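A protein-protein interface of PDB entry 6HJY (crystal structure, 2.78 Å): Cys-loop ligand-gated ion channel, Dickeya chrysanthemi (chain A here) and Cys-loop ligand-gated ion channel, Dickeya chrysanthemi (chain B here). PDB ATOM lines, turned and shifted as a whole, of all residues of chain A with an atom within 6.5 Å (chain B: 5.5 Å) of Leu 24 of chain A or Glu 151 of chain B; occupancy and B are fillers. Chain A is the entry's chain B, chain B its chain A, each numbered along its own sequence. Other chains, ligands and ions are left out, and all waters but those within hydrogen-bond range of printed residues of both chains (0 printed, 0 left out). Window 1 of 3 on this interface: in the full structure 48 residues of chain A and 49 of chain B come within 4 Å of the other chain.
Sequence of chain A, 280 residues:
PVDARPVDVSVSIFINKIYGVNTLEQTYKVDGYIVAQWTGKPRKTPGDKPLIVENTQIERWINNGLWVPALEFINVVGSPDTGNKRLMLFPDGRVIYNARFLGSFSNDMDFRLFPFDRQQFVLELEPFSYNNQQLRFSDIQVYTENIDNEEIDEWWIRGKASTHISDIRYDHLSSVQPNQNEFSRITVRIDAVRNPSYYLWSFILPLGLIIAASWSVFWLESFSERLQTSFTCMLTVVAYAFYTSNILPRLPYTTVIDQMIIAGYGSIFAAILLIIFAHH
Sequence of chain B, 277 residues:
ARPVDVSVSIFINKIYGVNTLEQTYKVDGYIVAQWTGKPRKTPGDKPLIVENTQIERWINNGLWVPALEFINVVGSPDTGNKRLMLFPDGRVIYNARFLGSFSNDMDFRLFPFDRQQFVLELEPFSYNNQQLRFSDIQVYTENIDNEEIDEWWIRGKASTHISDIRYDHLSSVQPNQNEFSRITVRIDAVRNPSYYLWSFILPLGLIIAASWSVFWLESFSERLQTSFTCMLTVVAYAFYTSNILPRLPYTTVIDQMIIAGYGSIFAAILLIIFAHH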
ATOM      1  N   ASN A  22      12.694 -17.800  -6.578  1.00  0.00           N
ATOM      2  CA  ASN A  22      12.004 -16.518  -6.649  1.00  0.00           C
ATOM      3  C   ASN A  22      13.008 -15.572  -7.282  1.00  0.00           C
ATOM      4  O   ASN A  22      13.954 -15.128  -6.621  1.00  0.00           O
ATOM      5  CB  ASN A  22      11.566 -16.026  -5.262  1.00  0.00           C
ATOM      6  CG  ASN A  22      10.782 -14.722  -5.261  1.00  0.00           C
ATOM      7  OD1 ASN A  22      11.081 -13.760  -5.983  1.00  0.00           O
ATOM      8  ND2 ASN A  22       9.793 -14.638  -4.389  1.00  0.00           N
ATOM      9  N   THR A  23      12.812 -15.310  -8.584  1.00  0.00           N
ATOM     10  CA  THR A  23      13.650 -14.483  -9.450  1.00  0.00           C
ATOM     11  C   THR A  23      13.897 -13.071  -8.929  1.00  0.00           C
ATOM     12  O   THR A  23      15.048 -12.630  -8.896  1.00  0.00           O
ATOM     13  CB  THR A  23      13.070 -14.436 -10.864  1.00  0.00           C
ATOM     14  OG1 THR A  23      11.690 -14.075 -10.792  1.00  0.00           O
ATOM     15  CG2 THR A  23      13.238 -15.750 -11.611  1.00  0.00           C
ATOM     16  N   LEU A  24      12.822 -12.367  -8.518  1.00  0.00           N
ATOM     17  CA  LEU A  24      12.908 -10.989  -8.030  1.00  0.00           C
ATOM     18  C   LEU A  24      13.611 -10.868  -6.677  1.00  0.00           C
ATOM     19  O   LEU A  24      14.405  -9.948  -6.485  1.00  0.00           O
ATOM     20  CB  LEU A  24      11.520 -10.321  -8.016  1.00  0.00           C
ATOM     21  CG  LEU A  24      11.484  -8.779  -8.045  1.00  0.00           C
ATOM     22  CD1 LEU A  24      12.377  -8.202  -9.152  1.00  0.00           C
ATOM     23  CD2 LEU A  24      10.063  -8.281  -8.231  1.00  0.00           C
ATOM     24  N   GLU A  25      13.340 -11.810  -5.753  1.00  0.00           N
ATOM     25  CA  GLU A  25      13.964 -11.842  -4.432  1.00  0.00           C
ATOM     26  C   GLU A  25      15.358 -12.461  -4.459  1.00  0.00           C
ATOM     27  O   GLU A  25      16.098 -12.307  -3.487  1.00  0.00           O
ATOM     28  CB  GLU A  25      13.087 -12.605  -3.438  1.00  0.00           C
ATOM     29  CG  GLU A  25      11.888 -11.814  -2.945  1.00  0.00           C
ATOM     30  CD  GLU A  25      11.102 -12.437  -1.800  1.00  0.00           C
ATOM     31  OE1 GLU A  25      11.413 -13.583  -1.400  1.00  0.00           O
ATOM     32  OE2 GLU A  25      10.163 -11.773  -1.306  1.00  0.00           O
ATOM     33  N   GLN A  26      15.713 -13.164  -5.568  1.00  0.00           N
ATOM     34  CA  GLN A  26      16.988 -13.875  -5.765  1.00  0.00           C
ATOM     35  C   GLN A  26      17.203 -14.915  -4.653  1.00  0.00           C
ATOM     36  O   GLN A  26      18.275 -14.989  -4.044  1.00  0.00           O
ATOM     37  CB  GLN A  26      18.180 -12.909  -5.924  1.00  0.00           C
ATOM     38  CG  GLN A  26      18.335 -12.357  -7.337  1.00  0.00           C
ATOM     39  CD  GLN A  26      19.448 -11.349  -7.402  1.00  0.00           C
ATOM     40  OE1 GLN A  26      20.622 -11.688  -7.549  1.00  0.00           O
ATOM     41  NE2 GLN A  26      19.103 -10.084  -7.267  1.00  0.00           N
ATOM     42  N   THR A  27      16.147 -15.715  -4.400  1.00  0.00           N
ATOM     43  CA  THR A  27      16.103 -16.781  -3.396  1.00  0.00           C
ATOM     44  C   THR A  27      15.663 -18.117  -4.015  1.00  0.00           C
ATOM     45  O   THR A  27      15.075 -18.134  -5.098  1.00  0.00           O
ATOM     46  CB  THR A  27      15.207 -16.387  -2.197  1.00  0.00           C
ATOM     47  OG1 THR A  27      13.883 -16.091  -2.644  1.00  0.00           O
ATOM     48  CG2 THR A  27      15.777 -15.228  -1.375  1.00  0.00           C
ATOM     49  N   PHE A 111      19.323 -13.562 -14.377  1.00  0.00           N
ATOM     50  CA  PHE A 111      18.356 -14.199 -15.270  1.00  0.00           C
ATOM     51  C   PHE A 111      18.249 -13.509 -16.636  1.00  0.00           C
ATOM     52  O   PHE A 111      17.268 -13.735 -17.341  1.00  0.00           O
ATOM     53  CB  PHE A 111      16.971 -14.255 -14.603  1.00  0.00           C
ATOM     54  CG  PHE A 111      16.918 -14.921 -13.251  1.00  0.00           C
ATOM     55  CD1 PHE A 111      16.783 -16.300 -13.142  1.00  0.00           C
ATOM     56  CD2 PHE A 111      16.953 -14.167 -12.086  1.00  0.00           C
ATOM     57  CE1 PHE A 111      16.717 -16.914 -11.889  1.00  0.00           C
ATOM     58  CE2 PHE A 111      16.879 -14.778 -10.837  1.00  0.00           C
ATOM     59  CZ  PHE A 111      16.756 -16.147 -10.745  1.00  0.00           C
ATOM     60  N   PRO A 249       8.665 -14.772 -15.263  1.00  0.00           N
ATOM     61  CA  PRO A 249       8.971 -14.295 -13.907  1.00  0.00           C
ATOM     62  C   PRO A 249       9.228 -12.794 -13.820  1.00  0.00           C
ATOM     63  O   PRO A 249       9.681 -12.188 -14.797  1.00  0.00           O
ATOM     64  CB  PRO A 249      10.215 -15.098 -13.538  1.00  0.00           C
ATOM     65  CG  PRO A 249      10.882 -15.381 -14.832  1.00  0.00           C
ATOM     66  CD  PRO A 249       9.767 -15.601 -15.804  1.00  0.00           C
ATOM     67  N   ARG A 250       8.958 -12.203 -12.636  1.00  0.00           N
ATOM     68  CA  ARG A 250       9.177 -10.776 -12.399  1.00  0.00           C
ATOM     69  C   ARG A 250      10.651 -10.450 -12.260  1.00  0.00           C
ATOM     70  O   ARG A 250      11.348 -11.060 -11.441  1.00  0.00           O
ATOM     71  CB  ARG A 250       8.338 -10.226 -11.230  1.00  0.00           C
ATOM     72  CG  ARG A 250       6.849 -10.026 -11.555  1.00  0.00           C
ATOM     73  CD  ARG A 250       6.552  -8.902 -12.557  1.00  0.00           C
ATOM     74  NE  ARG A 250       6.720  -9.355 -13.942  1.00  0.00           N
ATOM     75  CZ  ARG A 250       7.652  -8.908 -14.783  1.00  0.00           C
ATOM     76  NH1 ARG A 250       8.523  -7.986 -14.389  1.00  0.00           N
ATOM     77  NH2 ARG A 250       7.731  -9.393 -16.015  1.00  0.00           N
ATOM     78  N   LEU A 251      11.140  -9.534 -13.120  1.00  0.00           N
ATOM     79  CA  LEU A 251      12.547  -9.142 -13.177  1.00  0.00           C
ATOM     80  C   LEU A 251      12.766  -7.630 -13.374  1.00  0.00           C
ATOM     81  O   LEU A 251      11.956  -6.980 -14.043  1.00  0.00           O
ATOM     82  CB  LEU A 251      13.260  -9.937 -14.291  1.00  0.00           C
ATOM     83  CG  LEU A 251      13.522 -11.424 -14.014  1.00  0.00           C
ATOM     84  CD1 LEU A 251      13.848 -12.150 -15.280  1.00  0.00           C
ATOM     85  CD2 LEU A 251      14.638 -11.615 -12.997  1.00  0.00           C
ATOM     86  N   PRO A 252      13.876  -7.052 -12.839  1.00  0.00           N
ATOM     87  CA  PRO A 252      14.114  -5.609 -13.032  1.00  0.00           C
ATOM     88  C   PRO A 252      14.801  -5.261 -14.362  1.00  0.00           C
ATOM     89  O   PRO A 252      15.093  -4.091 -14.621  1.00  0.00           O
ATOM     90  CB  PRO A 252      14.993  -5.253 -11.836  1.00  0.00           C
ATOM     91  CG  PRO A 252      15.761  -6.490 -11.550  1.00  0.00           C
ATOM     92  CD  PRO A 252      14.952  -7.666 -12.028  1.00  0.00           C
ATOM     93  N   GLU B 147      25.275  -3.967  -9.954  1.00  0.00           N
ATOM     94  CA  GLU B 147      23.923  -3.513  -9.623  1.00  0.00           C
ATOM     95  C   GLU B 147      22.923  -3.690 -10.775  1.00  0.00           C
ATOM     96  O   GLU B 147      21.716  -3.549 -10.555  1.00  0.00           O
ATOM     97  CB  GLU B 147      23.941  -2.060  -9.110  1.00  0.00           C
ATOM     98  CG  GLU B 147      24.534  -1.050 -10.086  1.00  0.00           C
ATOM     99  CD  GLU B 147      24.316   0.418  -9.756  1.00  0.00           C
ATOM    100  OE1 GLU B 147      24.363   0.788  -8.561  1.00  0.00           O
ATOM    101  OE2 GLU B 147      24.142   1.213 -10.707  1.00  0.00           O
ATOM    102  N   ILE B 149      21.986  -6.401 -12.243  1.00  0.00           N
ATOM    103  CA  ILE B 149      21.157  -7.563 -11.910  1.00  0.00           C
ATOM    104  C   ILE B 149      20.227  -7.303 -10.696  1.00  0.00           C
ATOM    105  O   ILE B 149      19.405  -8.158 -10.365  1.00  0.00           O
ATOM    106  CB  ILE B 149      22.016  -8.865 -11.749  1.00  0.00           C
ATOM    107  CG1 ILE B 149      22.808  -8.899 -10.418  1.00  0.00           C
ATOM    108  CG2 ILE B 149      22.937  -9.088 -12.967  1.00  0.00           C
ATOM    109  CD1 ILE B 149      22.934 -10.274  -9.780  1.00  0.00           C
ATOM    110  N   ASP B 150      20.365  -6.129 -10.039  1.00  0.00           N
ATOM    111  CA  ASP B 150      19.584  -5.730  -8.862  1.00  0.00           C
ATOM    112  C   ASP B 150      18.427  -4.773  -9.183  1.00  0.00           C
ATOM    113  O   ASP B 150      18.558  -3.892 -10.038  1.00  0.00           O
ATOM    114  CB  ASP B 150      20.496  -5.103  -7.786  1.00  0.00           C
ATOM    115  CG  ASP B 150      21.579  -6.018  -7.245  1.00  0.00           C
ATOM    116  OD1 ASP B 150      21.280  -7.206  -6.988  1.00  0.00           O
ATOM    117  OD2 ASP B 150      22.708  -5.534  -7.028  1.00  0.00           O
ATOM    118  N   GLU B 151      17.311  -4.935  -8.444  1.00  0.00           N
ATOM    119  CA  GLU B 151      16.093  -4.129  -8.558  1.00  0.00           C
ATOM    120  C   GLU B 151      16.306  -2.698  -8.074  1.00  0.00           C
ATOM    121  O   GLU B 151      15.747  -1.766  -8.658  1.00  0.00           O
ATOM    122  CB  GLU B 151      14.937  -4.795  -7.793  1.00  0.00           C
ATOM    123  CG  GLU B 151      13.567  -4.210  -8.112  1.00  0.00           C
ATOM    124  CD  GLU B 151      12.376  -4.775  -7.352  1.00  0.00           C
ATOM    125  OE1 GLU B 151      12.557  -5.715  -6.543  1.00  0.00           O
ATOM    126  OE2 GLU B 151      11.250  -4.276  -7.575  1.00  0.00           O
ATOM    127  N   TRP B 152      17.100  -2.535  -6.998  1.00  0.00           N
ATOM    128  CA  TRP B 152      17.420  -1.246  -6.389  1.00  0.00           C
ATOM    129  C   TRP B 152      18.901  -0.929  -6.495  1.00  0.00           C
ATOM    130  O   TRP B 152      19.737  -1.838  -6.505  1.00  0.00           O
ATOM    131  CB  TRP B 152      16.958  -1.210  -4.924  1.00  0.00           C
ATOM    132  CG  TRP B 152      15.466  -1.187  -4.790  1.00  0.00           C
ATOM    133  CD1 TRP B 152      14.644  -2.255  -4.596  1.00  0.00           C
ATOM    134  CD2 TRP B 152      14.614  -0.041  -4.923  1.00  0.00           C
ATOM    135  NE1 TRP B 152      13.329  -1.845  -4.572  1.00  0.00           N
ATOM    136  CE2 TRP B 152      13.282  -0.488  -4.770  1.00  0.00           C
ATOM    137  CE3 TRP B 152      14.849   1.329  -5.131  1.00  0.00           C
ATOM    138  CZ2 TRP B 152      12.188   0.389  -4.820  1.00  0.00           C
ATOM    139  CZ3 TRP B 152      13.766   2.193  -5.194  1.00  0.00           C
ATOM    140  CH2 TRP B 152      12.454   1.721  -5.054  1.00  0.00           C
ATOM    141  N   TRP B 153      19.223   0.367  -6.590  1.00  0.00           N
ATOM    142  CA  TRP B 153      20.598   0.843  -6.686  1.00  0.00           C
ATOM    143  C   TRP B 153      20.918   1.755  -5.513  1.00  0.00           C
ATOM    144  O   TRP B 153      20.456   2.898  -5.475  1.00  0.00           O
ATOM    145  CB  TRP B 153      20.838   1.569  -8.016  1.00  0.00           C
ATOM    146  CG  TRP B 153      20.680   0.735  -9.258  1.00  0.00           C
ATOM    147  CD1 TRP B 153      20.732  -0.627  -9.358  1.00  0.00           C
ATOM    148  CD2 TRP B 153      20.505   1.230 -10.591  1.00  0.00           C
ATOM    149  NE1 TRP B 153      20.551  -1.013 -10.667  1.00  0.00           N
ATOM    150  CE2 TRP B 153      20.427   0.107 -11.449  1.00  0.00           C
ATOM    151  CE3 TRP B 153      20.402   2.517 -11.147  1.00  0.00           C
ATOM    152  CZ2 TRP B 153      20.268   0.239 -12.836  1.00  0.00           C
ATOM    153  CZ3 TRP B 153      20.217   2.644 -12.516  1.00  0.00           C
ATOM    154  CH2 TRP B 153      20.139   1.516 -13.344  1.00  0.00           C
ATOM    155  N   VAL B 190      17.843   4.144  -5.544  1.00  0.00           N
ATOM    156  CA  VAL B 190      17.152   4.574  -6.766  1.00  0.00           C
ATOM    157  C   VAL B 190      16.715   3.287  -7.471  1.00  0.00           C
ATOM    158  O   VAL B 190      17.484   2.323  -7.494  1.00  0.00           O
ATOM    159  CB  VAL B 190      18.082   5.441  -7.673  1.00  0.00           C
ATOM    160  CG1 VAL B 190      17.380   5.851  -8.965  1.00  0.00           C
ATOM    161  CG2 VAL B 190      18.583   6.680  -6.936  1.00  0.00           C
ATOM    162  N   ARG B 191      15.485   3.254  -8.017  1.00  0.00           N
ATOM    163  CA  ARG B 191      14.995   2.066  -8.721  1.00  0.00           C
ATOM    164  C   ARG B 191      15.710   1.867 -10.056  1.00  0.00           C
ATOM    165  O   ARG B 191      16.091   2.844 -10.705  1.00  0.00           O
ATOM    166  CB  ARG B 191      13.472   2.126  -8.934  1.00  0.00           C
ATOM    167  CG  ARG B 191      12.848   0.753  -9.224  1.00  0.00           C
ATOM    168  CD  ARG B 191      11.391   0.836  -9.625  1.00  0.00           C
ATOM    169  NE  ARG B 191      10.567   1.376  -8.544  1.00  0.00           N
ATOM    170  CZ  ARG B 191       9.996   0.653  -7.583  1.00  0.00           C
ATOM    171  NH1 ARG B 191      10.150  -0.668  -7.558  1.00  0.00           N
ATOM    172  NH2 ARG B 191       9.268   1.238  -6.645  1.00  0.00           N
ATOM    173  N   ASN B 192      15.916   0.591 -10.441  1.00  0.00           N
ATOM    174  CA  ASN B 192      16.496   0.194 -11.722  1.00  0.00           C
ATOM    175  C   ASN B 192      15.329   0.300 -12.732  1.00  0.00           C
ATOM    176  O   ASN B 192      14.390  -0.500 -12.654  1.00  0.00           O
ATOM    177  CB  ASN B 192      17.051  -1.252 -11.630  1.00  0.00           C
ATOM    178  CG  ASN B 192      17.710  -1.826 -12.870  1.00  0.00           C
ATOM    179  OD1 ASN B 192      17.635  -1.291 -13.981  1.00  0.00           O
ATOM    180  ND2 ASN B 192      18.410  -2.934 -12.692  1.00  0.00           N
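Among the printed residues, merely in contact across the chains: Leu 24 of chain A with Glu 151 of chain B (3.6 Å), Gln 26 of chain A with Ile 149 of chain B (3.5 Å), Gln 26 of chain A with Asp 150 of chain B (3.6 Å), Pro 252 of chain A with Asp 150 of chain B (3.96 Å), Pro 252 of chain A with Glu 151 of chain B (3.6 Å) and Pro 252 of chain A with Asn 192 of chain B (3.8 Å).
Leu 24 of chain A touches just one residue of chain B: Glu 151 (3.6 Å).
Of the printed residues of chain A, Asp 150 of chain B touches Gln 26 (3.6 Å) and Pro 252 (3.96 Å).
Printed residues of chain A within 4 Å of Ile 149 of chain B: Gln 26.
Of the printed residues of chain A, Asn 192 of chain B touches Pro 252 (3.8 Å).
Glu 147 of chain B touches none of the printed residues of chain A.
The nearest printed residue of chain B that does not touch Leu 24 of chain A is Ile 149 of chain B (6.6 Å).
The nearest residue of chain A that does not touch Glu 151 of chain B is Gln 26 of chain A (5.6 Å).
The nearest printed residue of chain B that does not touch Gln 26 of chain A is Glu 151 of chain B (5.6 Å).
Of the 9 printed residues of chain B, 4 touch a printed residue of chain A.
Hydrophobic or aromatic side chains of chain B that line the printed part of chain A: Ile 149.
Among the printed residues, no Asp or Glu carboxylate lies within 4 Å of a Lys or Arg side-chain nitrogen of the other chain.
O of Asp 150 of chain B sits at hydrogen-bond distance from ND2 of Asn 192 of chain B, at 2.8 Å.
OE2 of Glu 151 of chain B is in salt-bridge range of NH1 of Arg 191 of chain B.
O of Glu 151 of chain B lies within hydrogen-bond range of N of Asn 192 of chain B (3.0 Å).
OD1 of Asn 22 of chain A sits at hydrogen-bond distance from N of Leu 24 of chain A (3.4 Å).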
